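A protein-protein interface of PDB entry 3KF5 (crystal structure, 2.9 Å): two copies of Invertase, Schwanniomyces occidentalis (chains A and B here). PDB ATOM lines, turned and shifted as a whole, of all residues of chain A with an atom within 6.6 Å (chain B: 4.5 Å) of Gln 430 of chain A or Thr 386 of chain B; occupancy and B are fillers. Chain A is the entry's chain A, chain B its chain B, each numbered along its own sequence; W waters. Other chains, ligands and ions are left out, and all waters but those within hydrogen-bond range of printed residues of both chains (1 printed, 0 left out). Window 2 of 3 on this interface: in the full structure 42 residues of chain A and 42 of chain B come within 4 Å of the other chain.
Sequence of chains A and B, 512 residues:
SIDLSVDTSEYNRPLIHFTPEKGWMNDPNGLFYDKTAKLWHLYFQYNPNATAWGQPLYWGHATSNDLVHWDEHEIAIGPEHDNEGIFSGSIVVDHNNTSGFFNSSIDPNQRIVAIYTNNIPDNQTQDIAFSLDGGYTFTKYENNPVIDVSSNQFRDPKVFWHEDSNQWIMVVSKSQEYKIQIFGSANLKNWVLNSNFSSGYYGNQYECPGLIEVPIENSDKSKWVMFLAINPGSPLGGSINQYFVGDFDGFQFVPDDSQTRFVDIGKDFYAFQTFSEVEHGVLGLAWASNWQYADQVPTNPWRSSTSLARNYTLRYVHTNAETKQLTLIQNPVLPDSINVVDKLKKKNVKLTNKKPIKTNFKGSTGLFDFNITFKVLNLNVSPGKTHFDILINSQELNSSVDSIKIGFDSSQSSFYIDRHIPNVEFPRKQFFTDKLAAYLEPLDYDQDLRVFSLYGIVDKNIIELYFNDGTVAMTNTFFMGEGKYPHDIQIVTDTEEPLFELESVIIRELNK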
ATOM      1  N   GLN A 292     -15.759 -33.447 -19.088  1.00  0.00           N
ATOM      2  CA  GLN A 292     -15.069 -32.150 -19.070  1.00  0.00           C
ATOM      3  C   GLN A 292     -14.822 -31.507 -20.432  1.00  0.00           C
ATOM      4  O   GLN A 292     -14.507 -30.324 -20.506  1.00  0.00           O
ATOM      5  CB  GLN A 292     -13.782 -32.167 -18.226  1.00  0.00           C
ATOM      6  CG  GLN A 292     -12.912 -33.405 -18.318  1.00  0.00           C
ATOM      7  CD  GLN A 292     -11.774 -33.390 -17.310  1.00  0.00           C
ATOM      8  OE1 GLN A 292     -10.691 -33.906 -17.577  1.00  0.00           O
ATOM      9  NE2 GLN A 292     -12.010 -32.796 -16.152  1.00  0.00           N
ATOM     10  N   PHE A 426      -9.632 -26.891 -29.490  1.00  0.00           N
ATOM     11  CA  PHE A 426     -11.047 -26.758 -29.151  1.00  0.00           C
ATOM     12  C   PHE A 426     -11.206 -26.380 -27.677  1.00  0.00           C
ATOM     13  O   PHE A 426     -10.318 -26.669 -26.871  1.00  0.00           O
ATOM     14  CB  PHE A 426     -11.853 -28.021 -29.525  1.00  0.00           C
ATOM     15  CG  PHE A 426     -11.317 -29.301 -28.940  1.00  0.00           C
ATOM     16  CD1 PHE A 426     -10.423 -30.090 -29.660  1.00  0.00           C
ATOM     17  CD2 PHE A 426     -11.730 -29.739 -27.674  1.00  0.00           C
ATOM     18  CE1 PHE A 426      -9.923 -31.292 -29.125  1.00  0.00           C
ATOM     19  CE2 PHE A 426     -11.241 -30.936 -27.131  1.00  0.00           C
ATOM     20  CZ  PHE A 426     -10.334 -31.715 -27.862  1.00  0.00           C
ATOM     21  N   PRO A 427     -12.323 -25.713 -27.323  1.00  0.00           N
ATOM     22  CA  PRO A 427     -12.549 -25.296 -25.944  1.00  0.00           C
ATOM     23  C   PRO A 427     -12.375 -26.426 -24.939  1.00  0.00           C
ATOM     24  O   PRO A 427     -12.874 -27.527 -25.143  1.00  0.00           O
ATOM     25  CB  PRO A 427     -13.998 -24.829 -25.965  1.00  0.00           C
ATOM     26  CG  PRO A 427     -14.181 -24.314 -27.318  1.00  0.00           C
ATOM     27  CD  PRO A 427     -13.408 -25.241 -28.203  1.00  0.00           C
ATOM     28  N   ARG A 428     -11.632 -26.136 -23.879  1.00  0.00           N
ATOM     29  CA  ARG A 428     -11.422 -27.045 -22.752  1.00  0.00           C
ATOM     30  C   ARG A 428     -10.414 -28.198 -22.916  1.00  0.00           C
ATOM     31  O   ARG A 428     -10.338 -29.060 -22.046  1.00  0.00           O
ATOM     32  CB  ARG A 428     -12.749 -27.502 -22.130  1.00  0.00           C
ATOM     33  CG  ARG A 428     -13.496 -26.354 -21.471  1.00  0.00           C
ATOM     34  CD  ARG A 428     -14.546 -26.843 -20.522  1.00  0.00           C
ATOM     35  NE  ARG A 428     -15.905 -26.542 -20.971  1.00  0.00           N
ATOM     36  CZ  ARG A 428     -16.785 -27.443 -21.413  1.00  0.00           C
ATOM     37  NH1 ARG A 428     -16.459 -28.733 -21.486  1.00  0.00           N
ATOM     38  NH2 ARG A 428     -18.004 -27.053 -21.781  1.00  0.00           N
ATOM     39  N   LYS A 429      -9.644 -28.215 -24.009  1.00  0.00           N
ATOM     40  CA  LYS A 429      -8.349 -28.915 -23.987  1.00  0.00           C
ATOM     41  C   LYS A 429      -7.643 -28.298 -22.781  1.00  0.00           C
ATOM     42  O   LYS A 429      -7.930 -27.149 -22.454  1.00  0.00           O
ATOM     43  CB  LYS A 429      -7.535 -28.626 -25.239  1.00  0.00           C
ATOM     44  CG  LYS A 429      -8.034 -29.307 -26.496  1.00  0.00           C
ATOM     45  CD  LYS A 429      -7.110 -29.060 -27.705  1.00  0.00           C
ATOM     46  CE  LYS A 429      -5.966 -30.083 -27.806  1.00  0.00           C
ATOM     47  NZ  LYS A 429      -6.484 -31.458 -28.034  1.00  0.00           N
ATOM     48  N   GLN A 430      -6.732 -29.027 -22.140  1.00  0.00           N
ATOM     49  CA  GLN A 430      -6.265 -28.734 -20.760  1.00  0.00           C
ATOM     50  C   GLN A 430      -6.702 -29.917 -19.948  1.00  0.00           C
ATOM     51  O   GLN A 430      -5.996 -30.373 -19.052  1.00  0.00           O
ATOM     52  CB  GLN A 430      -6.932 -27.514 -20.112  1.00  0.00           C
ATOM     53  CG  GLN A 430      -6.340 -26.158 -20.425  1.00  0.00           C
ATOM     54  CD  GLN A 430      -7.424 -25.123 -20.754  1.00  0.00           C
ATOM     55  OE1 GLN A 430      -8.633 -25.397 -20.649  1.00  0.00           O
ATOM     56  NE2 GLN A 430      -6.992 -23.936 -21.183  1.00  0.00           N
ATOM     57  N   PHE A 431      -7.905 -30.391 -20.260  1.00  0.00           N
ATOM     58  CA  PHE A 431      -8.466 -31.563 -19.633  1.00  0.00           C
ATOM     59  C   PHE A 431      -8.333 -32.767 -20.572  1.00  0.00           C
ATOM     60  O   PHE A 431      -8.456 -33.915 -20.145  1.00  0.00           O
ATOM     61  CB  PHE A 431      -9.919 -31.284 -19.256  1.00  0.00           C
ATOM     62  CG  PHE A 431     -10.096 -30.079 -18.360  1.00  0.00           C
ATOM     63  CD1 PHE A 431     -10.780 -28.954 -18.806  1.00  0.00           C
ATOM     64  CD2 PHE A 431      -9.568 -30.065 -17.073  1.00  0.00           C
ATOM     65  CE1 PHE A 431     -10.945 -27.828 -17.981  1.00  0.00           C
ATOM     66  CE2 PHE A 431      -9.724 -28.945 -16.240  1.00  0.00           C
ATOM     67  CZ  PHE A 431     -10.416 -27.825 -16.698  1.00  0.00           C
ATOM     68  N   PHE A 432      -8.055 -32.490 -21.843  1.00  0.00           N
ATOM     69  CA  PHE A 432      -7.888 -33.517 -22.865  1.00  0.00           C
ATOM     70  C   PHE A 432      -6.461 -34.092 -22.790  1.00  0.00           C
ATOM     71  O   PHE A 432      -5.518 -33.485 -23.314  1.00  0.00           O
ATOM     72  CB  PHE A 432      -8.188 -32.915 -24.249  1.00  0.00           C
ATOM     73  CG  PHE A 432      -8.480 -33.940 -25.306  1.00  0.00           C
ATOM     74  CD1 PHE A 432      -9.768 -34.448 -25.466  1.00  0.00           C
ATOM     75  CD2 PHE A 432      -7.466 -34.413 -26.136  1.00  0.00           C
ATOM     76  CE1 PHE A 432     -10.043 -35.416 -26.444  1.00  0.00           C
ATOM     77  CE2 PHE A 432      -7.731 -35.378 -27.112  1.00  0.00           C
ATOM     78  CZ  PHE A 432      -9.024 -35.880 -27.267  1.00  0.00           C
ATOM     79  N   THR A 433      -6.313 -35.272 -22.180  1.00  0.00           N
ATOM     80  CA  THR A 433      -5.034 -35.663 -21.564  1.00  0.00           C
ATOM     81  C   THR A 433      -3.814 -36.071 -22.427  1.00  0.00           C
ATOM     82  O   THR A 433      -2.659 -35.761 -22.046  1.00  0.00           O
ATOM     83  CB  THR A 433      -5.240 -36.583 -20.343  1.00  0.00           C
ATOM     84  OG1 THR A 433      -5.684 -35.783 -19.246  1.00  0.00           O
ATOM     85  CG2 THR A 433      -3.939 -37.278 -19.923  1.00  0.00           C
ATOM     86  N   GLY B 384     -15.094 -21.694 -24.683  1.00  0.00           N
ATOM     87  CA  GLY B 384     -13.656 -21.808 -24.616  1.00  0.00           C
ATOM     88  C   GLY B 384     -13.021 -20.660 -23.878  1.00  0.00           C
ATOM     89  O   GLY B 384     -13.237 -20.457 -22.679  1.00  0.00           O
ATOM     90  N   LYS B 385     -12.248 -19.882 -24.616  1.00  0.00           N
ATOM     91  CA  LYS B 385     -11.361 -18.902 -24.012  1.00  0.00           C
ATOM     92  C   LYS B 385     -10.182 -19.690 -23.408  1.00  0.00           C
ATOM     93  O   LYS B 385      -9.273 -20.113 -24.149  1.00  0.00           O
ATOM     94  CB  LYS B 385     -12.112 -18.020 -22.976  1.00  0.00           C
ATOM     95  CG  LYS B 385     -12.619 -16.629 -23.480  1.00  0.00           C
ATOM     96  CD  LYS B 385     -13.361 -16.613 -24.838  1.00  0.00           C
ATOM     97  CE  LYS B 385     -12.597 -15.858 -25.928  1.00  0.00           C
ATOM     98  NZ  LYS B 385     -11.580 -16.709 -26.614  1.00  0.00           N
ATOM     99  N   THR B 386     -10.231 -19.902 -22.087  1.00  0.00           N
ATOM    100  CA  THR B 386      -9.215 -20.614 -21.296  1.00  0.00           C
ATOM    101  C   THR B 386      -9.255 -20.103 -19.861  1.00  0.00           C
ATOM    102  O   THR B 386      -8.216 -19.797 -19.275  1.00  0.00           O
ATOM    103  CB  THR B 386      -7.765 -20.475 -21.855  1.00  0.00           C
ATOM    104  OG1 THR B 386      -6.874 -21.288 -21.076  1.00  0.00           O
ATOM    105  CG2 THR B 386      -7.272 -19.004 -21.856  1.00  0.00           C
ATOM    106  N   HIS B 387     -10.465 -20.037 -19.305  1.00  0.00           N
ATOM    107  CA  HIS B 387     -10.770 -19.275 -18.082  1.00  0.00           C
ATOM    108  C   HIS B 387      -9.536 -19.105 -17.182  1.00  0.00           C
ATOM    109  O   HIS B 387      -8.969 -20.094 -16.729  1.00  0.00           O
ATOM    110  CB  HIS B 387     -11.980 -19.904 -17.364  1.00  0.00           C
ATOM    111  CG  HIS B 387     -13.182 -20.092 -18.251  1.00  0.00           C
ATOM    112  ND1 HIS B 387     -13.516 -19.208 -19.263  1.00  0.00           N
ATOM    113  CD2 HIS B 387     -14.130 -21.062 -18.275  1.00  0.00           C
ATOM    114  CE1 HIS B 387     -14.613 -19.631 -19.869  1.00  0.00           C
ATOM    115  NE2 HIS B 387     -15.005 -20.753 -19.290  1.00  0.00           N
ATOM    116  N   PHE B 388      -9.127 -17.851 -16.970  1.00  0.00           N
ATOM    117  CA  PHE B 388      -7.794 -17.422 -16.416  1.00  0.00           C
ATOM    118  C   PHE B 388      -6.630 -18.412 -16.105  1.00  0.00           C
ATOM    119  O   PHE B 388      -6.792 -19.401 -15.394  1.00  0.00           O
ATOM    120  CB  PHE B 388      -7.967 -16.368 -15.289  1.00  0.00           C
ATOM    121  CG  PHE B 388      -7.657 -16.864 -13.901  1.00  0.00           C
ATOM    122  CD1 PHE B 388      -6.377 -16.746 -13.377  1.00  0.00           C
ATOM    123  CD2 PHE B 388      -8.649 -17.414 -13.103  1.00  0.00           C
ATOM    124  CE1 PHE B 388      -6.085 -17.199 -12.089  1.00  0.00           C
ATOM    125  CE2 PHE B 388      -8.363 -17.868 -11.809  1.00  0.00           C
ATOM    126  CZ  PHE B 388      -7.082 -17.759 -11.305  1.00  0.00           C
ATOM    127  N   ASP B 389      -5.446 -18.091 -16.628  1.00  0.00           N
ATOM    128  CA  ASP B 389      -4.222 -18.871 -16.388  1.00  0.00           C
ATOM    129  C   ASP B 389      -3.112 -18.027 -15.771  1.00  0.00           C
ATOM    130  O   ASP B 389      -3.028 -16.818 -16.001  1.00  0.00           O
ATOM    131  CB  ASP B 389      -3.666 -19.464 -17.685  1.00  0.00           C
ATOM    132  CG  ASP B 389      -4.736 -20.016 -18.576  1.00  0.00           C
ATOM    133  OD1 ASP B 389      -5.447 -19.202 -19.205  1.00  0.00           O
ATOM    134  OD2 ASP B 389      -4.847 -21.262 -18.662  1.00  0.00           O
ATOM    135  N   LYS B 405       2.253 -23.735 -17.415  1.00  0.00           N
ATOM    136  CA  LYS B 405       0.957 -23.077 -17.292  1.00  0.00           C
ATOM    137  C   LYS B 405       0.129 -23.657 -16.137  1.00  0.00           C
ATOM    138  O   LYS B 405      -0.024 -24.872 -16.023  1.00  0.00           O
ATOM    139  CB  LYS B 405       0.225 -23.221 -18.627  1.00  0.00           C
ATOM    140  CG  LYS B 405      -1.024 -22.373 -18.819  1.00  0.00           C
ATOM    141  CD  LYS B 405      -1.392 -22.268 -20.318  1.00  0.00           C
ATOM    142  CE  LYS B 405      -2.047 -23.553 -20.894  1.00  0.00           C
ATOM    143  NZ  LYS B 405      -3.516 -23.660 -20.603  1.00  0.00           N
ATOM    144  N   TYR B 416      -5.770 -26.675 -13.069  1.00  0.00           N
ATOM    145  CA  TYR B 416      -5.023 -27.524 -13.994  1.00  0.00           C
ATOM    146  C   TYR B 416      -3.601 -27.034 -14.247  1.00  0.00           C
ATOM    147  O   TYR B 416      -3.311 -25.842 -14.132  1.00  0.00           O
ATOM    148  CB  TYR B 416      -5.767 -27.633 -15.318  1.00  0.00           C
ATOM    149  CG  TYR B 416      -6.002 -26.301 -15.984  1.00  0.00           C
ATOM    150  CD1 TYR B 416      -5.018 -25.712 -16.785  1.00  0.00           C
ATOM    151  CD2 TYR B 416      -7.207 -25.633 -15.826  1.00  0.00           C
ATOM    152  CE1 TYR B 416      -5.231 -24.492 -17.405  1.00  0.00           C
ATOM    153  CE2 TYR B 416      -7.432 -24.412 -16.444  1.00  0.00           C
ATOM    154  CZ  TYR B 416      -6.441 -23.845 -17.229  1.00  0.00           C
ATOM    155  OH  TYR B 416      -6.666 -22.628 -17.835  1.00  0.00           O
ATOM    156  N   LYS B 435      -0.535 -32.688 -18.656  1.00  0.00           N
ATOM    157  CA  LYS B 435      -1.809 -32.045 -18.284  1.00  0.00           C
ATOM    158  C   LYS B 435      -2.528 -32.750 -17.142  1.00  0.00           C
ATOM    159  O   LYS B 435      -2.875 -33.927 -17.255  1.00  0.00           O
ATOM    160  CB  LYS B 435      -2.741 -31.971 -19.489  1.00  0.00           C
ATOM    161  CG  LYS B 435      -2.202 -31.156 -20.642  1.00  0.00           C
ATOM    162  CD  LYS B 435      -3.187 -31.132 -21.770  1.00  0.00           C
ATOM    163  CE  LYS B 435      -2.665 -30.317 -22.926  1.00  0.00           C
ATOM    164  NZ  LYS B 435      -3.799 -29.942 -23.820  1.00  0.00           N
ATOM    165  N   ASP B 494      -8.517 -14.429 -21.631  1.00  0.00           N
ATOM    166  CA  ASP B 494      -9.005 -14.043 -22.949  1.00  0.00           C
ATOM    167  C   ASP B 494     -10.350 -13.316 -22.874  1.00  0.00           C
ATOM    168  O   ASP B 494     -10.845 -12.834 -23.890  1.00  0.00           O
ATOM    169  CB  ASP B 494      -9.114 -15.261 -23.872  1.00  0.00           C
ATOM    170  CG  ASP B 494      -7.765 -15.871 -24.207  1.00  0.00           C
ATOM    171  OD1 ASP B 494      -6.743 -15.160 -24.158  1.00  0.00           O
ATOM    172  OD2 ASP B 494      -7.730 -17.074 -24.534  1.00  0.00           O
HETATM  173  O   HOH W   1      -4.047 -27.130 -23.133  1.00  0.00           O
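The side-chain amide nitrogen of Gln 430 of chain A lies within hydrogen-bond range of the side-chain hydroxyl of Thr 386 of chain B.
The side-chain amide oxygen (OE1) of Gln 292 of chain A sits close to the backbone carbonyl oxygen (O) of Phe 431 of chain A.
OG1 of Thr 433 of chain A lies within hydrogen-bond range of O of Phe 431 of chain A (3.5 Å).
The side-chain hydroxyl (OG1) of Thr 386 of chain B lies within hydrogen-bond range of the side-chain carboxylate (OD1) of Asp 389 of chain B, at 3.1 Å.
The side-chain carboxylate (OD2) of Asp 389 of chain B lies within salt-bridge range of the side-chain amino group (NZ) of Lys 405 of chain B (3.4 Å).
The side-chain hydroxyl of Tyr 416 of chain B lies within hydrogen-bond range of the side-chain carboxylate of Asp 389 of chain B (2.4 Å).
Pro 427 of chain A touches Gly 384 of chain B.
Gln 430 of chain A touches Lys 405 of chain B.
NE2 of Gln 430 of chain A touches OH of Tyr 416 of chain B, 3.6 Å away.
Gln 430 of chain A touches Lys 435 of chain B (N to NZ, 3.5 Å).
Phe 431 of chain A touches Tyr 416 of chain B (CZ to CD2, 3.98 Å).
Lys 435 of chain B touches Phe 432 of chain A (CD to O, 3.7 Å).
Thr 433 of chain A touches Lys 435 of chain B (OG1 to O, 3.9 Å).
Thr 386 of chain B touches just one residue of chain A: Gln 430.
Printed residues of chain B within 4 Å of Pro 427 of chain A: Gly 384 (3.3 Å).
Printed residues of chain A within 4 Å of Tyr 416 of chain B: Gln 430 (3.6 Å) and Phe 431 (3.98 Å).
Of the printed residues of chain B, Thr 433 of chain A touches Lys 435.
Of the printed residues of chain B, Phe 432 of chain A touches Lys 435 (3.7 Å).
Of the printed residues of chain A, Lys 405 of chain B touches Gln 430 (3.5 Å).
The nearest residue of chain B that does not touch Gln 430 of chain A is Asp 389 of chain B (4.3 Å).
The nearest printed residue of chain A that does not touch Tyr 416 of chain B is Lys 429 of chain A (6.3 Å).
Hydrophobic or aromatic side chains of chain B within 4 Å of the printed part of chain A: Tyr 416.
Printed residues of chain A that touch a printed residue of chain B: Pro 427, Gln 430, Phe 431, Phe 432 and Thr 433.
Hydrophobic or aromatic side chains of chain A within 4 Å of the printed part of chain B: Pro 427 and Phe 431.
Among the printed residues, 8 pairs touch across the chains.
Among the printed residues, no Asp or Glu carboxylate lies within 4 Å of a Lys or Arg side-chain nitrogen of the other chain.
No position is printed for both chains.
Of the 8 pairs that touch across the chains among the printed residues, none has its exchanged pair printed and touching as well.
Water W1 lies within hydrogen-bond range of the side-chain amino group (NZ) of Lys 435 of chain B and the backbone NH (N) of Gln 430 of chain A.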
